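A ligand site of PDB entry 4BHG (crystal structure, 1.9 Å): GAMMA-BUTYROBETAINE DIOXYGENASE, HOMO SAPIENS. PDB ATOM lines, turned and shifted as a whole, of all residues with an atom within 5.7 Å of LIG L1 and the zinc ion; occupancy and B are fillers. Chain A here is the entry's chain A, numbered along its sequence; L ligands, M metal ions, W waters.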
ATOM      1  N   TRP A 181     -33.291  16.258  20.771  1.00  0.00           N
ATOM      2  CA  TRP A 181     -32.553  16.621  21.994  1.00  0.00           C
ATOM      3  C   TRP A 181     -32.072  18.052  21.886  1.00  0.00           C
ATOM      4  O   TRP A 181     -31.914  18.600  20.783  1.00  0.00           O
ATOM      5  CB  TRP A 181     -31.389  15.666  22.256  1.00  0.00           C
ATOM      6  CG  TRP A 181     -30.852  14.976  21.048  1.00  0.00           C
ATOM      7  CD1 TRP A 181     -31.214  13.734  20.582  1.00  0.00           C
ATOM      8  CD2 TRP A 181     -29.852  15.461  20.130  1.00  0.00           C
ATOM      9  NE1 TRP A 181     -30.530  13.440  19.438  1.00  0.00           N
ATOM     10  CE2 TRP A 181     -29.695  14.480  19.139  1.00  0.00           C
ATOM     11  CE3 TRP A 181     -29.109  16.633  20.047  1.00  0.00           C
ATOM     12  CZ2 TRP A 181     -28.798  14.618  18.090  1.00  0.00           C
ATOM     13  CZ3 TRP A 181     -28.214  16.770  19.007  1.00  0.00           C
ATOM     14  CH2 TRP A 181     -28.083  15.768  18.018  1.00  0.00           C
ATOM     15  N   VAL A 183     -29.333  20.917  22.645  1.00  0.00           N
ATOM     16  CA  VAL A 183     -27.941  21.222  22.904  1.00  0.00           C
ATOM     17  C   VAL A 183     -27.901  22.601  23.547  1.00  0.00           C
ATOM     18  O   VAL A 183     -28.088  23.608  22.872  1.00  0.00           O
ATOM     19  CB  VAL A 183     -27.063  21.202  21.628  1.00  0.00           C
ATOM     20  CG1 VAL A 183     -25.588  21.348  21.987  1.00  0.00           C
ATOM     21  CG2 VAL A 183     -27.307  19.940  20.817  1.00  0.00           C
ATOM     22  N   ALA A 193     -21.385  17.675  25.378  1.00  0.00           N
ATOM     23  CA  ALA A 193     -22.059  18.539  24.438  1.00  0.00           C
ATOM     24  C   ALA A 193     -23.032  19.512  25.131  1.00  0.00           C
ATOM     25  O   ALA A 193     -23.293  20.599  24.599  1.00  0.00           O
ATOM     26  CB  ALA A 193     -22.780  17.695  23.384  1.00  0.00           C
ATOM     27  N   TYR A 194     -23.521  19.153  26.319  1.00  0.00           N
ATOM     28  CA  TYR A 194     -24.489  19.966  27.072  1.00  0.00           C
ATOM     29  C   TYR A 194     -23.768  20.876  28.101  1.00  0.00           C
ATOM     30  O   TYR A 194     -24.213  21.016  29.242  1.00  0.00           O
ATOM     31  CB  TYR A 194     -25.480  19.060  27.788  1.00  0.00           C
ATOM     32  CG  TYR A 194     -26.297  18.161  26.849  1.00  0.00           C
ATOM     33  CD1 TYR A 194     -26.585  18.567  25.523  1.00  0.00           C
ATOM     34  CD2 TYR A 194     -26.835  16.976  27.307  1.00  0.00           C
ATOM     35  CE1 TYR A 194     -27.348  17.765  24.690  1.00  0.00           C
ATOM     36  CE2 TYR A 194     -27.603  16.144  26.460  1.00  0.00           C
ATOM     37  CZ  TYR A 194     -27.883  16.572  25.169  1.00  0.00           C
ATOM     38  OH  TYR A 194     -28.631  15.789  24.320  1.00  0.00           O
ATOM     39  N   LEU A 199     -16.038  21.535  21.578  1.00  0.00           N
ATOM     40  CA  LEU A 199     -16.051  20.164  21.129  1.00  0.00           C
ATOM     41  C   LEU A 199     -15.045  20.090  19.997  1.00  0.00           C
ATOM     42  O   LEU A 199     -15.199  20.795  18.971  1.00  0.00           O
ATOM     43  CB  LEU A 199     -17.459  19.761  20.630  1.00  0.00           C
ATOM     44  CG  LEU A 199     -18.592  19.888  21.661  1.00  0.00           C
ATOM     45  CD1 LEU A 199     -19.925  19.469  21.045  1.00  0.00           C
ATOM     46  CD2 LEU A 199     -18.286  19.074  22.904  1.00  0.00           C
ATOM     47  N   HIS A 202     -15.309  15.422  16.135  1.00  0.00           N
ATOM     48  CA  HIS A 202     -15.791  14.085  16.490  1.00  0.00           C
ATOM     49  C   HIS A 202     -16.903  13.663  15.548  1.00  0.00           C
ATOM     50  O   HIS A 202     -17.455  14.498  14.813  1.00  0.00           O
ATOM     51  CB  HIS A 202     -16.310  14.090  17.921  1.00  0.00           C
ATOM     52  CG  HIS A 202     -17.474  15.011  18.134  1.00  0.00           C
ATOM     53  ND1 HIS A 202     -17.344  16.377  18.177  1.00  0.00           N
ATOM     54  CD2 HIS A 202     -18.792  14.756  18.263  1.00  0.00           C
ATOM     55  CE1 HIS A 202     -18.531  16.930  18.340  1.00  0.00           C
ATOM     56  NE2 HIS A 202     -19.427  15.955  18.380  1.00  0.00           N
ATOM     57  N   THR A 203     -17.208  12.363  15.568  1.00  0.00           N
ATOM     58  CA  THR A 203     -18.458  11.851  15.080  1.00  0.00           C
ATOM     59  C   THR A 203     -19.368  11.575  16.279  1.00  0.00           C
ATOM     60  O   THR A 203     -18.897  11.349  17.400  1.00  0.00           O
ATOM     61  CB  THR A 203     -18.275  10.536  14.262  1.00  0.00           C
ATOM     62  OG1 THR A 203     -17.682   9.512  15.084  1.00  0.00           O
ATOM     63  CG2 THR A 203     -17.407  10.760  13.037  1.00  0.00           C
ATOM     64  N   ASP A 204     -20.675  11.638  16.066  1.00  0.00           N
ATOM     65  CA  ASP A 204     -21.621  11.437  17.148  1.00  0.00           C
ATOM     66  C   ASP A 204     -21.861   9.943  17.356  1.00  0.00           C
ATOM     67  O   ASP A 204     -22.071   9.194  16.413  1.00  0.00           O
ATOM     68  CB  ASP A 204     -22.959  12.104  16.877  1.00  0.00           C
ATOM     69  CG  ASP A 204     -23.051  13.497  17.497  1.00  0.00           C
ATOM     70  OD1 ASP A 204     -22.032  14.171  17.504  1.00  0.00           O
ATOM     71  OD2 ASP A 204     -24.144  13.866  17.980  1.00  0.00           O
ATOM     72  N   GLN A 215     -27.061  13.327  10.812  1.00  0.00           N
ATOM     73  CA  GLN A 215     -27.379  14.158  11.935  1.00  0.00           C
ATOM     74  C   GLN A 215     -28.014  15.447  11.447  1.00  0.00           C
ATOM     75  O   GLN A 215     -27.603  16.000  10.432  1.00  0.00           O
ATOM     76  CB  GLN A 215     -26.108  14.447  12.741  1.00  0.00           C
ATOM     77  CG  GLN A 215     -26.327  15.239  14.021  1.00  0.00           C
ATOM     78  CD  GLN A 215     -25.086  15.301  14.903  1.00  0.00           C
ATOM     79  OE1 GLN A 215     -24.913  16.219  15.736  1.00  0.00           O
ATOM     80  NE2 GLN A 215     -24.209  14.327  14.735  1.00  0.00           N
ATOM     81  N   LEU A 217     -28.990  19.369  12.903  1.00  0.00           N
ATOM     82  CA  LEU A 217     -28.865  20.342  13.967  1.00  0.00           C
ATOM     83  C   LEU A 217     -29.535  21.642  13.565  1.00  0.00           C
ATOM     84  O   LEU A 217     -29.156  22.239  12.546  1.00  0.00           O
ATOM     85  CB  LEU A 217     -27.392  20.641  14.288  1.00  0.00           C
ATOM     86  CG  LEU A 217     -26.558  19.588  15.025  1.00  0.00           C
ATOM     87  CD1 LEU A 217     -25.120  20.080  15.188  1.00  0.00           C
ATOM     88  CD2 LEU A 217     -27.184  19.309  16.372  1.00  0.00           C
ATOM     89  N   GLY A 227     -19.077  29.581  19.903  1.00  0.00           N
ATOM     90  CA  GLY A 227     -20.043  28.584  19.383  1.00  0.00           C
ATOM     91  C   GLY A 227     -20.118  28.442  17.877  1.00  0.00           C
ATOM     92  O   GLY A 227     -21.105  27.913  17.352  1.00  0.00           O
ATOM     93  N   ASP A 228     -19.090  28.906  17.172  1.00  0.00           N
ATOM     94  CA  ASP A 228     -18.943  28.632  15.754  1.00  0.00           C
ATOM     95  C   ASP A 228     -18.831  27.125  15.502  1.00  0.00           C
ATOM     96  O   ASP A 228     -18.329  26.376  16.345  1.00  0.00           O
ATOM     97  CB  ASP A 228     -17.666  29.260  15.180  1.00  0.00           C
ATOM     98  CG  ASP A 228     -17.570  30.727  15.472  1.00  0.00           C
ATOM     99  OD1 ASP A 228     -17.385  31.049  16.660  1.00  0.00           O
ATOM    100  OD2 ASP A 228     -17.687  31.526  14.506  1.00  0.00           O
ATOM    101  N   SER A 229     -19.235  26.723  14.301  1.00  0.00           N
ATOM    102  CA  SER A 229     -19.200  25.341  13.875  1.00  0.00           C
ATOM    103  C   SER A 229     -17.966  25.088  13.014  1.00  0.00           C
ATOM    104  O   SER A 229     -17.419  25.991  12.326  1.00  0.00           O
ATOM    105  CB  SER A 229     -20.460  24.995  13.077  1.00  0.00           C
ATOM    106  OG  SER A 229     -21.619  25.167  13.846  1.00  0.00           O
ATOM    107  N   HIS A 347     -17.306  16.827  13.089  1.00  0.00           N
ATOM    108  CA  HIS A 347     -17.779  18.161  13.375  1.00  0.00           C
ATOM    109  C   HIS A 347     -17.337  18.589  14.765  1.00  0.00           C
ATOM    110  O   HIS A 347     -16.926  17.782  15.631  1.00  0.00           O
ATOM    111  CB  HIS A 347     -19.299  18.246  13.202  1.00  0.00           C
ATOM    112  CG  HIS A 347     -20.080  17.382  14.154  1.00  0.00           C
ATOM    113  ND1 HIS A 347     -20.204  16.021  13.978  1.00  0.00           N
ATOM    114  CD2 HIS A 347     -20.778  17.681  15.263  1.00  0.00           C
ATOM    115  CE1 HIS A 347     -20.929  15.511  14.956  1.00  0.00           C
ATOM    116  NE2 HIS A 347     -21.278  16.496  15.773  1.00  0.00           N
ATOM    117  N   GLY A 348     -17.388  19.894  14.963  1.00  0.00           N
ATOM    118  CA  GLY A 348     -16.980  20.470  16.222  1.00  0.00           C
ATOM    119  C   GLY A 348     -17.648  21.788  16.465  1.00  0.00           C
ATOM    120  O   GLY A 348     -18.368  22.312  15.617  1.00  0.00           O
ATOM    121  N   ARG A 349     -17.347  22.335  17.621  1.00  0.00           N
ATOM    122  CA  ARG A 349     -17.877  23.601  18.031  1.00  0.00           C
ATOM    123  C   ARG A 349     -16.870  24.343  18.902  1.00  0.00           C
ATOM    124  O   ARG A 349     -16.214  23.767  19.781  1.00  0.00           O
ATOM    125  CB  ARG A 349     -19.149  23.383  18.819  1.00  0.00           C
ATOM    126  CG  ARG A 349     -19.501  24.427  19.837  1.00  0.00           C
ATOM    127  CD  ARG A 349     -20.578  23.916  20.754  1.00  0.00           C
ATOM    128  NE  ARG A 349     -20.113  23.429  22.026  1.00  0.00           N
ATOM    129  CZ  ARG A 349     -20.862  22.701  22.833  1.00  0.00           C
ATOM    130  NH1 ARG A 349     -22.079  22.332  22.459  1.00  0.00           N
ATOM    131  NH2 ARG A 349     -20.389  22.307  24.001  1.00  0.00           N
ATOM    132  N   ARG A 360     -27.685  29.990  24.049  1.00  0.00           N
ATOM    133  CA  ARG A 360     -27.418  29.162  22.893  1.00  0.00           C
ATOM    134  C   ARG A 360     -28.212  27.860  23.045  1.00  0.00           C
ATOM    135  O   ARG A 360     -28.183  27.234  24.107  1.00  0.00           O
ATOM    136  CB  ARG A 360     -25.927  28.832  22.778  1.00  0.00           C
ATOM    137  CG  ARG A 360     -25.540  28.220  21.423  1.00  0.00           C
ATOM    138  CD  ARG A 360     -24.057  27.921  21.392  1.00  0.00           C
ATOM    139  NE  ARG A 360     -23.589  27.501  20.076  1.00  0.00           N
ATOM    140  CZ  ARG A 360     -23.495  26.243  19.635  1.00  0.00           C
ATOM    141  NH1 ARG A 360     -23.887  25.215  20.353  1.00  0.00           N
ATOM    142  NH2 ARG A 360     -23.005  26.021  18.426  1.00  0.00           N
ATOM    143  N   LEU A 362     -29.486  24.608  20.342  1.00  0.00           N
ATOM    144  CA  LEU A 362     -29.751  23.884  19.097  1.00  0.00           C
ATOM    145  C   LEU A 362     -30.677  22.720  19.444  1.00  0.00           C
ATOM    146  O   LEU A 362     -30.559  22.143  20.523  1.00  0.00           O
ATOM    147  CB  LEU A 362     -28.483  23.319  18.497  1.00  0.00           C
ATOM    148  CG  LEU A 362     -27.206  24.143  18.429  1.00  0.00           C
ATOM    149  CD1 LEU A 362     -26.101  23.286  17.813  1.00  0.00           C
ATOM    150  CD2 LEU A 362     -27.458  25.385  17.634  1.00  0.00           C
ATOM    151  N   TYR A 366     -31.252  12.427  14.829  1.00  0.00           N
ATOM    152  CA  TYR A 366     -30.513  11.513  13.987  1.00  0.00           C
ATOM    153  C   TYR A 366     -31.458  10.802  13.031  1.00  0.00           C
ATOM    154  O   TYR A 366     -32.645  10.662  13.298  1.00  0.00           O
ATOM    155  CB  TYR A 366     -29.839  10.440  14.856  1.00  0.00           C
ATOM    156  CG  TYR A 366     -28.815  10.986  15.849  1.00  0.00           C
ATOM    157  CD1 TYR A 366     -27.721  11.727  15.404  1.00  0.00           C
ATOM    158  CD2 TYR A 366     -28.911  10.686  17.198  1.00  0.00           C
ATOM    159  CE1 TYR A 366     -26.779  12.213  16.308  1.00  0.00           C
ATOM    160  CE2 TYR A 366     -27.953  11.118  18.091  1.00  0.00           C
ATOM    161  CZ  TYR A 366     -26.881  11.876  17.631  1.00  0.00           C
ATOM    162  OH  TYR A 366     -25.953  12.329  18.559  1.00  0.00           O
HETATM  163  C1  LIG L   1     -23.085  17.637  19.541  1.00  0.00           C
HETATM  164  C2  LIG L   1     -22.427  18.679  18.749  1.00  0.00           C
HETATM  165  C3  LIG L   1     -22.459  20.989  17.972  1.00  0.00           C
HETATM  166  C4  LIG L   1     -22.734  22.377  18.523  1.00  0.00           C
HETATM  167  O1  LIG L   1     -23.973  18.047  20.330  1.00  0.00           O
HETATM  168  O2  LIG L   1     -22.757  16.405  19.340  1.00  0.00           O
HETATM  169  O3  LIG L   1     -21.540  18.349  17.977  1.00  0.00           O
HETATM  170  O4  LIG L   1     -22.492  23.333  17.780  1.00  0.00           O
HETATM  171  N1  LIG L   1     -22.880  19.920  18.876  1.00  0.00           N
HETATM  172  O5  LIG L   1     -23.149  22.515  19.692  1.00  0.00           O
HETATM  173  C1  LG2 L   2     -22.083  11.346  21.668  1.00  0.00           C
HETATM  174  N1  LG2 L   2     -24.542  13.518  21.362  1.00  0.00           N
HETATM  175  O1  LG2 L   2     -22.031  11.710  22.867  1.00  0.00           O
HETATM  176  C2  LG2 L   2     -23.392  11.351  20.920  1.00  0.00           C
HETATM  177  N2  LG2 L   2     -25.564  14.384  21.835  1.00  0.00           N
HETATM  178  O2  LG2 L   2     -21.098  10.904  21.067  1.00  0.00           O
HETATM  179  C3  LG2 L   2     -24.550  12.077  21.614  1.00  0.00           C
HETATM  180  C4  LG2 L   2     -25.383  15.735  21.288  1.00  0.00           C
HETATM  181  C5  LG2 L   2     -25.549  14.498  23.313  1.00  0.00           C
HETATM  182  C6  LG2 L   2     -26.866  14.074  21.237  1.00  0.00           C
HETATM  183  C7  LG2 L   2     -27.491  12.860  21.731  1.00  0.00           C
HETATM  184 ZN    ZN M   1     -21.585  16.163  17.810  1.00  0.00          ZN
HETATM  185  O   HOH W   1     -21.421  22.892  15.282  1.00  0.00           O
HETATM  186  O   HOH W   2     -21.670  14.382  21.022  1.00  0.00           O
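NE2 of Gln 215 lies close to OD2 of Asp 204 (3.3 Å).
The side-chain carboxylate (OD2) of Asp 204 lies within hydrogen-bond range of the side-chain hydroxyl (OH) of Tyr 366 (2.4 Å).
The guanidinium group (NH2) of Arg 360 sits at hydrogen-bond distance from the backbone carbonyl oxygen (O) of Gly 227 (2.9 Å).
O of Ala 193 sits at hydrogen-bond distance from NH1 of Arg 349 (3.0 Å).
O of Arg 349 sits at hydrogen-bond distance from N of Leu 199 (2.9 Å).
The backbone NH (N) of Val 183 sits at hydrogen-bond distance from the backbone carbonyl oxygen (O) of Leu 362 (2.7 Å).
Val 183 touches LIG L1.
Ala 193 touches LIG L1.
Leu 199 touches LIG L1 (CD1 to C2, 3.5 Å).
Leu 217 touches LIG L1 (CD1 to C3, 3.96 Å).
Leu 362 touches LIG L1 (CD1 to C4, 3.6 Å).
Within 4 Å of LIG L1: Val 183, Ala 193, Leu 199, His 202, Asp 204, Leu 217, His 347, Arg 349, Arg 360 and Leu 362.
The nearest printed residue that does not touch LIG L1 is Gln 215 (4.2 Å).
Water W1 lies within hydrogen-bond range of the side-chain hydroxyl (OG) of Ser 229 (2.7 Å), an oxygen (O4) of LIG L1 (2.8 Å) and the backbone carbonyl oxygen (O) of Gly 348 (3.1 Å).
The zinc ion is bound by O2 of LIG L1, OD1 of Asp 204, NE2 of His 347, O3 of LIG L1 and NE2 of His 202.
O4 of LIG L1 is in salt-bridge range of NH2 of Arg 360 (2.8 Å).
An oxygen (O5) of LIG L1 is in salt-bridge range of the guanidinium group of Arg 349 (3.0 Å).
A nitrogen (N1) of LG2 L2 is in hydrogen-bond range of the side-chain carboxylate (OD2) of Asp 204 (3.4 Å).
OH of Tyr 366 sits close to N1 of LG2 L2, at 3.4 Å.
Gln 215 touches the zinc ion (OE1 to ZN, 3.9 Å).
Four residues have an atom within 4 Å of the zinc ion: His 202, Asp 204, Gln 215 and His 347.
Along chain A the residues within 4 Å of the zinc ion span positions 202 to 347.
The nearest printed residue that does not touch the zinc ion is Leu 199 (4.9 Å).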
